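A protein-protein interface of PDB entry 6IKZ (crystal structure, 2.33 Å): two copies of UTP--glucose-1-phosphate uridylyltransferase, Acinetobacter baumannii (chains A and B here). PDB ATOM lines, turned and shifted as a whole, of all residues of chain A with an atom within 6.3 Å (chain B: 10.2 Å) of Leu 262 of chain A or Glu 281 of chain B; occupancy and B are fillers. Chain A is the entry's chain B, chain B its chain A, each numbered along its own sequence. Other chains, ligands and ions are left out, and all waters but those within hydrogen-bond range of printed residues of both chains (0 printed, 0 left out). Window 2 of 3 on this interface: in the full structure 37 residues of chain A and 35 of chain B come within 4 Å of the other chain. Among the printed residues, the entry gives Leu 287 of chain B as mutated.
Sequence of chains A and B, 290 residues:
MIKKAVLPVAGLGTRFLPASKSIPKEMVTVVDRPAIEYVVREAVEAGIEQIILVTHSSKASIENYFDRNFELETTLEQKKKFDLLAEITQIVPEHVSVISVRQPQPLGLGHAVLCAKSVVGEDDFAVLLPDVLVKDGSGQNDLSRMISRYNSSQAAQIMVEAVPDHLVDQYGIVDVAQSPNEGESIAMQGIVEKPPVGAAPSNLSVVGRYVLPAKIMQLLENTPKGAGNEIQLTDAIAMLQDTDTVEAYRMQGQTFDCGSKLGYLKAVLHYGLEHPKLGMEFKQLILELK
Hydrophobic or aromatic side chains of chain A that line the printed part of chain B: Phe 16, Leu 262, Tyr 264 and Leu 265. Along chain A the printed residues that touch a printed residue of chain B span positions 16 to 265. Hydrophobic or aromatic side chains of chain B within 4 Å of the printed part of chain A: Leu 278, Phe 282 and Leu 285.
The side-chain carboxylate of Asp 32 of chain B is in hydrogen-bond range of a ring nitrogen (NE2) of His 275 of chain B. The backbone NH (N) of Leu 278 of chain B sits at hydrogen-bond distance from a ring nitrogen (ND1) of His 275 of chain B.
No residue of chain B comes within 4 Å of Ser 260 of chain A. Of chain B, only Leu 278 (3.5 Å), Glu 281 (3.8 Å) and Leu 285 (3.9 Å) come within 4 Å of Leu 262 of chain A. No residue of chain B comes within 4 Å of Gly 263 of chain A. Printed residues of chain B within 4 Å of Tyr 264 of chain A: Val 31 (3.3 Å). Of chain B, only Val 31 (3.9 Å) and Phe 282 (3.97 Å) come within 4 Å of Leu 265 of chain A. Of the printed residues of chain A, Val 31 of chain B touches Phe 16 (3.5 Å), Tyr 264 (3.3 Å) and Leu 265 (3.9 Å). Of the printed residues of chain A, Leu 278 of chain B touches Leu 262 (3.5 Å). Lys 283 of chain B touches none of the printed residues of chain A. Ile 286 of chain B touches none of the printed residues of chain A. The nearest residue of chain B that does not touch Leu 262 of chain A is Phe 282 of chain B (5.0 Å). The nearest printed residue of chain A that does not touch Glu 281 of chain B is Leu 265 of chain A (7.4 Å). The nearest printed residue of chain B that does not touch Tyr 264 of chain A is Asp 32 of chain B (5.3 Å).
No position is printed for both chains.
NZ of Lys 261 of chain A lies within salt-bridge range of OD2 of Asp 32 of chain B (3.6 Å).
Among the printed residues, pairs that only touch across the chains: Tyr 264 of chain A with Val 31 of chain B, Phe 16 of chain A with Val 31 of chain B, Leu 262 of chain A with Leu 278 of chain B, Leu 262 of chain A with Glu 281 of chain B, Leu 262 of chain A with Leu 285 of chain B, Leu 265 of chain A with Val 31 of chain B and Leu 265 of chain A with Phe 282 of chain B.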
ATOM      1  N   PHE A  16      -3.245  34.057 -26.507  1.00  0.00           N
ATOM      2  CA  PHE A  16      -2.158  33.149 -26.970  1.00  0.00           C
ATOM      3  C   PHE A  16      -0.845  33.523 -26.276  1.00  0.00           C
ATOM      4  O   PHE A  16       0.075  34.090 -26.877  1.00  0.00           O
ATOM      5  CB  PHE A  16      -2.091  33.016 -28.501  1.00  0.00           C
ATOM      6  CG  PHE A  16      -1.486  31.694 -28.930  1.00  0.00           C
ATOM      7  CD1 PHE A  16      -1.833  30.513 -28.283  1.00  0.00           C
ATOM      8  CD2 PHE A  16      -0.520  31.629 -29.920  1.00  0.00           C
ATOM      9  CE1 PHE A  16      -1.242  29.306 -28.622  1.00  0.00           C
ATOM     10  CE2 PHE A  16       0.067  30.420 -30.259  1.00  0.00           C
ATOM     11  CZ  PHE A  16      -0.295  29.263 -29.614  1.00  0.00           C
ATOM     12  N   ASP A 257      -9.281  30.436 -35.388  1.00  0.00           N
ATOM     13  CA  ASP A 257      -8.944  31.554 -34.477  1.00  0.00           C
ATOM     14  C   ASP A 257      -7.564  31.188 -33.953  1.00  0.00           C
ATOM     15  O   ASP A 257      -7.502  30.244 -33.162  1.00  0.00           O
ATOM     16  CB  ASP A 257     -10.033  31.749 -33.419  1.00  0.00           C
ATOM     17  CG  ASP A 257      -9.766  32.820 -32.367  1.00  0.00           C
ATOM     18  OD1 ASP A 257      -9.049  33.804 -32.658  1.00  0.00           O
ATOM     19  OD2 ASP A 257     -10.301  32.664 -31.246  1.00  0.00           O
ATOM     20  N   SER A 260      -7.034  31.504 -30.004  1.00  0.00           N
ATOM     21  CA  SER A 260      -7.228  30.352 -29.079  1.00  0.00           C
ATOM     22  C   SER A 260      -6.177  29.256 -29.347  1.00  0.00           C
ATOM     23  O   SER A 260      -5.902  28.934 -30.530  1.00  0.00           O
ATOM     24  CB  SER A 260      -8.635  29.812 -29.134  1.00  0.00           C
ATOM     25  OG  SER A 260      -8.821  28.944 -30.234  1.00  0.00           O
ATOM     26  N   LYS A 261      -5.635  28.669 -28.273  1.00  0.00           N
ATOM     27  CA  LYS A 261      -4.556  27.646 -28.330  1.00  0.00           C
ATOM     28  C   LYS A 261      -5.019  26.482 -29.214  1.00  0.00           C
ATOM     29  O   LYS A 261      -4.176  25.967 -29.961  1.00  0.00           O
ATOM     30  CB  LYS A 261      -4.142  27.196 -26.924  1.00  0.00           C
ATOM     31  CG  LYS A 261      -3.554  28.291 -26.047  1.00  0.00           C
ATOM     32  CD  LYS A 261      -2.605  27.778 -24.993  1.00  0.00           C
ATOM     33  CE  LYS A 261      -2.040  28.885 -24.123  1.00  0.00           C
ATOM     34  NZ  LYS A 261      -1.303  28.352 -22.947  1.00  0.00           N
ATOM     35  N   LEU A 262      -6.306  26.112 -29.185  1.00  0.00           N
ATOM     36  CA  LEU A 262      -6.813  24.939 -29.957  1.00  0.00           C
ATOM     37  C   LEU A 262      -7.090  25.330 -31.412  1.00  0.00           C
ATOM     38  O   LEU A 262      -6.829  24.527 -32.304  1.00  0.00           O
ATOM     39  CB  LEU A 262      -8.050  24.346 -29.287  1.00  0.00           C
ATOM     40  CG  LEU A 262      -7.890  22.868 -28.935  1.00  0.00           C
ATOM     41  CD1 LEU A 262      -7.007  22.694 -27.700  1.00  0.00           C
ATOM     42  CD2 LEU A 262      -9.243  22.194 -28.744  1.00  0.00           C
ATOM     43  N   GLY A 263      -7.563  26.542 -31.659  1.00  0.00           N
ATOM     44  CA  GLY A 263      -7.750  27.022 -33.035  1.00  0.00           C
ATOM     45  C   GLY A 263      -6.422  27.123 -33.749  1.00  0.00           C
ATOM     46  O   GLY A 263      -6.408  26.871 -34.954  1.00  0.00           O
ATOM     47  N   TYR A 264      -5.338  27.471 -33.040  1.00  0.00           N
ATOM     48  CA  TYR A 264      -3.974  27.567 -33.634  1.00  0.00           C
ATOM     49  C   TYR A 264      -3.468  26.139 -33.903  1.00  0.00           C
ATOM     50  O   TYR A 264      -2.988  25.851 -35.019  1.00  0.00           O
ATOM     51  CB  TYR A 264      -3.042  28.450 -32.793  1.00  0.00           C
ATOM     52  CG  TYR A 264      -1.578  28.145 -32.970  1.00  0.00           C
ATOM     53  CD1 TYR A 264      -1.000  27.105 -32.274  1.00  0.00           C
ATOM     54  CD2 TYR A 264      -0.777  28.850 -33.858  1.00  0.00           C
ATOM     55  CE1 TYR A 264       0.334  26.779 -32.434  1.00  0.00           C
ATOM     56  CE2 TYR A 264       0.564  28.520 -34.047  1.00  0.00           C
ATOM     57  CZ  TYR A 264       1.133  27.485 -33.318  1.00  0.00           C
ATOM     58  OH  TYR A 264       2.449  27.090 -33.455  1.00  0.00           O
ATOM     59  N   LEU A 265      -3.634  25.208 -32.965  1.00  0.00           N
ATOM     60  CA  LEU A 265      -3.201  23.801 -33.208  1.00  0.00           C
ATOM     61  C   LEU A 265      -4.014  23.197 -34.375  1.00  0.00           C
ATOM     62  O   LEU A 265      -3.539  22.267 -35.030  1.00  0.00           O
ATOM     63  CB  LEU A 265      -3.338  22.981 -31.915  1.00  0.00           C
ATOM     64  CG  LEU A 265      -2.464  23.397 -30.728  1.00  0.00           C
ATOM     65  CD1 LEU A 265      -0.994  23.133 -31.037  1.00  0.00           C
ATOM     66  N   LYS A 266      -5.217  23.686 -34.650  1.00  0.00           N
ATOM     67  CA  LYS A 266      -6.038  23.137 -35.750  1.00  0.00           C
ATOM     68  C   LYS A 266      -5.534  23.732 -37.047  1.00  0.00           C
ATOM     69  O   LYS A 266      -5.584  23.034 -38.062  1.00  0.00           O
ATOM     70  CB  LYS A 266      -7.521  23.431 -35.557  1.00  0.00           C
ATOM     71  CG  LYS A 266      -8.466  22.656 -36.471  1.00  0.00           C
ATOM     72  CD  LYS A 266      -9.847  23.303 -36.610  1.00  0.00           C
ATOM     73  CE  LYS A 266     -10.946  22.309 -36.947  1.00  0.00           C
ATOM     74  NZ  LYS A 266     -11.963  22.898 -37.852  1.00  0.00           N
ATOM     75  N   ALA A 267      -5.046  24.964 -37.016  1.00  0.00           N
ATOM     76  CA  ALA A 267      -4.495  25.652 -38.214  1.00  0.00           C
ATOM     77  C   ALA A 267      -3.196  24.978 -38.685  1.00  0.00           C
ATOM     78  O   ALA A 267      -2.989  24.839 -39.882  1.00  0.00           O
ATOM     79  CB  ALA A 267      -4.257  27.118 -37.914  1.00  0.00           C
ATOM     80  N   VAL B  31       3.818  24.327 -29.903  1.00  0.00           N
ATOM     81  CA  VAL B  31       2.496  24.156 -29.218  1.00  0.00           C
ATOM     82  C   VAL B  31       1.993  25.521 -28.722  1.00  0.00           C
ATOM     83  O   VAL B  31       1.009  26.048 -29.281  1.00  0.00           O
ATOM     84  CB  VAL B  31       2.539  23.138 -28.060  1.00  0.00           C
ATOM     85  CG1 VAL B  31       1.148  22.668 -27.679  1.00  0.00           C
ATOM     86  CG2 VAL B  31       3.395  21.929 -28.368  1.00  0.00           C
ATOM     87  N   ASP B  32       2.601  26.069 -27.678  1.00  0.00           N
ATOM     88  CA  ASP B  32       2.073  27.266 -26.975  1.00  0.00           C
ATOM     89  C   ASP B  32       3.196  28.127 -26.372  1.00  0.00           C
ATOM     90  O   ASP B  32       2.859  29.155 -25.763  1.00  0.00           O
ATOM     91  CB  ASP B  32       1.087  26.819 -25.896  1.00  0.00           C
ATOM     92  CG  ASP B  32       1.670  25.961 -24.782  1.00  0.00           C
ATOM     93  OD1 ASP B  32       2.887  25.673 -24.809  1.00  0.00           O
ATOM     94  OD2 ASP B  32       0.899  25.604 -23.873  1.00  0.00           O
ATOM     95  N   GLY B 272       2.664  18.605 -28.171  1.00  0.00           N
ATOM     96  CA  GLY B 272       1.197  18.744 -28.234  1.00  0.00           C
ATOM     97  C   GLY B 272       0.498  17.594 -27.529  1.00  0.00           C
ATOM     98  O   GLY B 272      -0.244  17.878 -26.584  1.00  0.00           O
ATOM     99  N   LEU B 273       0.761  16.342 -27.936  1.00  0.00           N
ATOM    100  CA  LEU B 273       0.097  15.123 -27.382  1.00  0.00           C
ATOM    101  C   LEU B 273       0.320  15.043 -25.872  1.00  0.00           C
ATOM    102  O   LEU B 273      -0.614  14.632 -25.184  1.00  0.00           O
ATOM    103  CB  LEU B 273       0.634  13.848 -28.050  1.00  0.00           C
ATOM    104  CG  LEU B 273       0.178  13.572 -29.487  1.00  0.00           C
ATOM    105  CD1 LEU B 273      -1.338  13.609 -29.599  1.00  0.00           C
ATOM    106  N   GLU B 274       1.509  15.424 -25.406  1.00  0.00           N
ATOM    107  CA  GLU B 274       1.984  15.247 -24.010  1.00  0.00           C
ATOM    108  C   GLU B 274       1.678  16.517 -23.214  1.00  0.00           C
ATOM    109  O   GLU B 274       1.940  16.546 -21.996  1.00  0.00           O
ATOM    110  CB  GLU B 274       3.484  14.946 -24.017  1.00  0.00           C
ATOM    111  CG  GLU B 274       3.997  14.230 -22.779  1.00  0.00           C
ATOM    112  CD  GLU B 274       5.507  14.327 -22.606  1.00  0.00           C
ATOM    113  OE1 GLU B 274       6.035  15.469 -22.635  1.00  0.00           O
ATOM    114  OE2 GLU B 274       6.162  13.266 -22.456  1.00  0.00           O
ATOM    115  N   HIS B 275       1.136  17.544 -23.867  1.00  0.00           N
ATOM    116  CA  HIS B 275       0.801  18.826 -23.198  1.00  0.00           C
ATOM    117  C   HIS B 275      -0.185  18.555 -22.071  1.00  0.00           C
ATOM    118  O   HIS B 275      -1.232  17.929 -22.259  1.00  0.00           O
ATOM    119  CB  HIS B 275       0.252  19.845 -24.189  1.00  0.00           C
ATOM    120  CG  HIS B 275       0.118  21.211 -23.609  1.00  0.00           C
ATOM    121  ND1 HIS B 275      -0.969  21.585 -22.872  1.00  0.00           N
ATOM    122  CD2 HIS B 275       0.923  22.295 -23.679  1.00  0.00           C
ATOM    123  CE1 HIS B 275      -0.835  22.844 -22.509  1.00  0.00           C
ATOM    124  NE2 HIS B 275       0.312  23.305 -23.007  1.00  0.00           N
ATOM    125  N   PRO B 276       0.118  19.073 -20.870  1.00  0.00           N
ATOM    126  CA  PRO B 276      -0.649  18.683 -19.690  1.00  0.00           C
ATOM    127  C   PRO B 276      -2.142  19.062 -19.742  1.00  0.00           C
ATOM    128  O   PRO B 276      -2.870  18.473 -18.988  1.00  0.00           O
ATOM    129  CB  PRO B 276       0.107  19.430 -18.580  1.00  0.00           C
ATOM    130  CG  PRO B 276       1.224  20.153 -19.319  1.00  0.00           C
ATOM    131  N   LYS B 277      -2.550  19.998 -20.612  1.00  0.00           N
ATOM    132  CA  LYS B 277      -3.930  20.575 -20.672  1.00  0.00           C
ATOM    133  C   LYS B 277      -4.584  20.377 -22.046  1.00  0.00           C
ATOM    134  O   LYS B 277      -5.791  20.096 -22.079  1.00  0.00           O
ATOM    135  CB  LYS B 277      -3.928  22.081 -20.389  1.00  0.00           C
ATOM    136  CG  LYS B 277      -3.324  22.475 -19.049  1.00  0.00           C
ATOM    137  CD  LYS B 277      -4.250  23.258 -18.143  1.00  0.00           C
ATOM    138  CE  LYS B 277      -4.231  22.723 -16.725  1.00  0.00           C
ATOM    139  NZ  LYS B 277      -4.027  23.816 -15.749  1.00  0.00           N
ATOM    140  N   LEU B 278      -3.826  20.516 -23.136  1.00  0.00           N
ATOM    141  CA  LEU B 278      -4.346  20.433 -24.528  1.00  0.00           C
ATOM    142  C   LEU B 278      -4.182  19.029 -25.080  1.00  0.00           C
ATOM    143  O   LEU B 278      -4.839  18.743 -26.076  1.00  0.00           O
ATOM    144  CB  LEU B 278      -3.558  21.402 -25.401  1.00  0.00           C
ATOM    145  CG  LEU B 278      -3.469  22.815 -24.851  1.00  0.00           C
ATOM    146  CD1 LEU B 278      -2.292  23.550 -25.475  1.00  0.00           C
ATOM    147  CD2 LEU B 278      -4.795  23.537 -25.075  1.00  0.00           C
ATOM    148  N   GLY B 279      -3.258  18.237 -24.527  1.00  0.00           N
ATOM    149  CA  GLY B 279      -2.905  16.913 -25.075  1.00  0.00           C
ATOM    150  C   GLY B 279      -4.146  16.190 -25.561  1.00  0.00           C
ATOM    151  O   GLY B 279      -4.222  15.869 -26.745  1.00  0.00           O
ATOM    152  N   MET B 280      -5.134  16.022 -24.689  1.00  0.00           N
ATOM    153  CA  MET B 280      -6.303  15.162 -24.976  1.00  0.00           C
ATOM    154  C   MET B 280      -7.169  15.804 -26.063  1.00  0.00           C
ATOM    155  O   MET B 280      -7.622  15.065 -26.961  1.00  0.00           O
ATOM    156  CB  MET B 280      -7.116  14.924 -23.704  1.00  0.00           C
ATOM    157  CG  MET B 280      -6.361  14.121 -22.650  1.00  0.00           C
ATOM    158  SD  MET B 280      -6.803  12.350 -22.658  1.00  0.00           S
ATOM    159  CE  MET B 280      -5.796  11.735 -24.007  1.00  0.00           C
ATOM    160  N   GLU B 281      -7.382  17.119 -26.008  1.00  0.00           N
ATOM    161  CA  GLU B 281      -8.218  17.828 -27.015  1.00  0.00           C
ATOM    162  C   GLU B 281      -7.443  17.880 -28.336  1.00  0.00           C
ATOM    163  O   GLU B 281      -8.094  17.980 -29.382  1.00  0.00           O
ATOM    164  CB  GLU B 281      -8.623  19.221 -26.528  1.00  0.00           C
ATOM    165  CG  GLU B 281      -9.667  19.197 -25.426  1.00  0.00           C
ATOM    166  CD  GLU B 281      -9.926  20.513 -24.698  1.00  0.00           C
ATOM    167  OE1 GLU B 281      -8.939  21.222 -24.353  1.00  0.00           O
ATOM    168  OE2 GLU B 281     -11.123  20.817 -24.449  1.00  0.00           O
ATOM    169  N   PHE B 282      -6.109  17.794 -28.288  1.00  0.00           N
ATOM    170  CA  PHE B 282      -5.217  17.854 -29.478  1.00  0.00           C
ATOM    171  C   PHE B 282      -5.193  16.502 -30.173  1.00  0.00           C
ATOM    172  O   PHE B 282      -5.322  16.489 -31.358  1.00  0.00           O
ATOM    173  CB  PHE B 282      -3.790  18.251 -29.108  1.00  0.00           C
ATOM    174  CG  PHE B 282      -2.814  18.261 -30.255  1.00  0.00           C
ATOM    175  CD1 PHE B 282      -3.031  19.060 -31.362  1.00  0.00           C
ATOM    176  CD2 PHE B 282      -1.642  17.528 -30.194  1.00  0.00           C
ATOM    177  CE1 PHE B 282      -2.105  19.104 -32.393  1.00  0.00           C
ATOM    178  CE2 PHE B 282      -0.717  17.563 -31.229  1.00  0.00           C
ATOM    179  CZ  PHE B 282      -0.948  18.357 -32.324  1.00  0.00           C
ATOM    180  N   LYS B 283      -5.027  15.411 -29.436  1.00  0.00           N
ATOM    181  CA  LYS B 283      -5.335  14.053 -29.938  1.00  0.00           C
ATOM    182  C   LYS B 283      -6.681  14.079 -30.679  1.00  0.00           C
ATOM    183  O   LYS B 283      -6.759  13.498 -31.779  1.00  0.00           O
ATOM    184  CB  LYS B 283      -5.381  13.068 -28.774  1.00  0.00           C
ATOM    185  CG  LYS B 283      -5.826  11.655 -29.136  1.00  0.00           C
ATOM    186  CD  LYS B 283      -6.506  10.931 -27.980  1.00  0.00           C
ATOM    187  CE  LYS B 283      -6.050   9.497 -27.791  1.00  0.00           C
ATOM    188  NZ  LYS B 283      -6.112   9.101 -26.363  1.00  0.00           N
ATOM    189  N   GLN B 284      -7.696  14.742 -30.121  1.00  0.00           N
ATOM    190  CA  GLN B 284      -9.069  14.772 -30.698  1.00  0.00           C
ATOM    191  C   GLN B 284      -9.013  15.402 -32.096  1.00  0.00           C
ATOM    192  O   GLN B 284      -9.616  14.828 -33.032  1.00  0.00           O
ATOM    193  CB  GLN B 284     -10.037  15.509 -29.765  1.00  0.00           C
ATOM    194  CG  GLN B 284     -11.501  15.145 -29.976  1.00  0.00           C
ATOM    195  CD  GLN B 284     -11.799  13.698 -29.649  1.00  0.00           C
ATOM    196  OE1 GLN B 284     -11.624  13.245 -28.514  1.00  0.00           O
ATOM    197  NE2 GLN B 284     -12.259  12.962 -30.651  1.00  0.00           N
ATOM    198  N   LEU B 285      -8.293  16.517 -32.240  1.00  0.00           N
ATOM    199  CA  LEU B 285      -8.097  17.219 -33.540  1.00  0.00           C
ATOM    200  C   LEU B 285      -7.452  16.288 -34.573  1.00  0.00           C
ATOM    201  O   LEU B 285      -7.865  16.383 -35.744  1.00  0.00           O
ATOM    202  CB  LEU B 285      -7.230  18.461 -33.333  1.00  0.00           C
ATOM    203  CG  LEU B 285      -7.888  19.577 -32.526  1.00  0.00           C
ATOM    204  CD1 LEU B 285      -6.872  20.642 -32.156  1.00  0.00           C
ATOM    205  CD2 LEU B 285      -9.045  20.198 -33.291  1.00  0.00           C
ATOM    206  N   ILE B 286      -6.481  15.450 -34.163  1.00  0.00           N
ATOM    207  CA  ILE B 286      -5.788  14.456 -35.041  1.00  0.00           C
ATOM    208  C   ILE B 286      -6.802  13.424 -35.544  1.00  0.00           C
ATOM    209  O   ILE B 286      -6.938  13.303 -36.765  1.00  0.00           O
ATOM    210  CB  ILE B 286      -4.623  13.762 -34.317  1.00  0.00           C
ATOM    211  CG1 ILE B 286      -3.283  14.369 -34.720  1.00  0.00           C
ATOM    212  CD1 ILE B 286      -2.849  15.488 -33.812  1.00  0.00           C
ATOM    213  N   LEU B 287      -7.480  12.714 -34.635  1.00  0.00           N
ATOM    214  CA  LEU B 287      -8.501  11.667 -34.961  1.00  0.00           C
ATOM    215  C   LEU B 287      -9.454  12.180 -36.055  1.00  0.00           C
ATOM    216  O   LEU B 287      -9.695  11.456 -37.020  1.00  0.00           O
ATOM    217  CB  LEU B 287      -9.285  11.291 -33.693  1.00  0.00           C
ATOM    218  CG  LEU B 287      -8.502  10.601 -32.572  1.00  0.00           C
ATOM    219  CD1 LEU B 287      -7.663   9.429 -33.078  1.00  0.00           C
ATOM    220  N   GLU B 288      -9.932  13.414 -35.923  1.00  0.00           N
ATOM    221  CA  GLU B 288     -10.960  14.024 -36.804  1.00  0.00           C
ATOM    222  C   GLU B 288     -10.386  14.278 -38.206  1.00  0.00           C
ATOM    223  O   GLU B 288     -11.167  14.705 -39.056  1.00  0.00           O
ATOM    224  CB  GLU B 288     -11.496  15.313 -36.165  1.00  0.00           C
ATOM    225  CG  GLU B 288     -12.228  15.082 -34.843  1.00  0.00           C
ATOM    226  CD  GLU B 288     -12.508  16.309 -33.981  1.00  0.00           C
ATOM    227  OE1 GLU B 288     -12.084  17.420 -34.367  1.00  0.00           O
ATOM    228  OE2 GLU B 288     -13.157  16.155 -32.921  1.00  0.00           O
ATOM    229  N   LEU B 289      -9.107  13.992 -38.469  1.00  0.00           N
ATOM    230  CA  LEU B 289      -8.419  14.424 -39.726  1.00  0.00           C
ATOM    231  C   LEU B 289      -8.902  13.630 -40.959  1.00  0.00           C
ATOM    232  O   LEU B 289      -8.548  14.046 -42.097  1.00  0.00           O
ATOM    233  CB  LEU B 289      -6.897  14.313 -39.558  1.00  0.00           C
ATOM    234  CG  LEU B 289      -6.214  15.486 -38.853  1.00  0.00           C
ATOM    235  CD1 LEU B 289      -6.181  16.702 -39.766  1.00  0.00           C
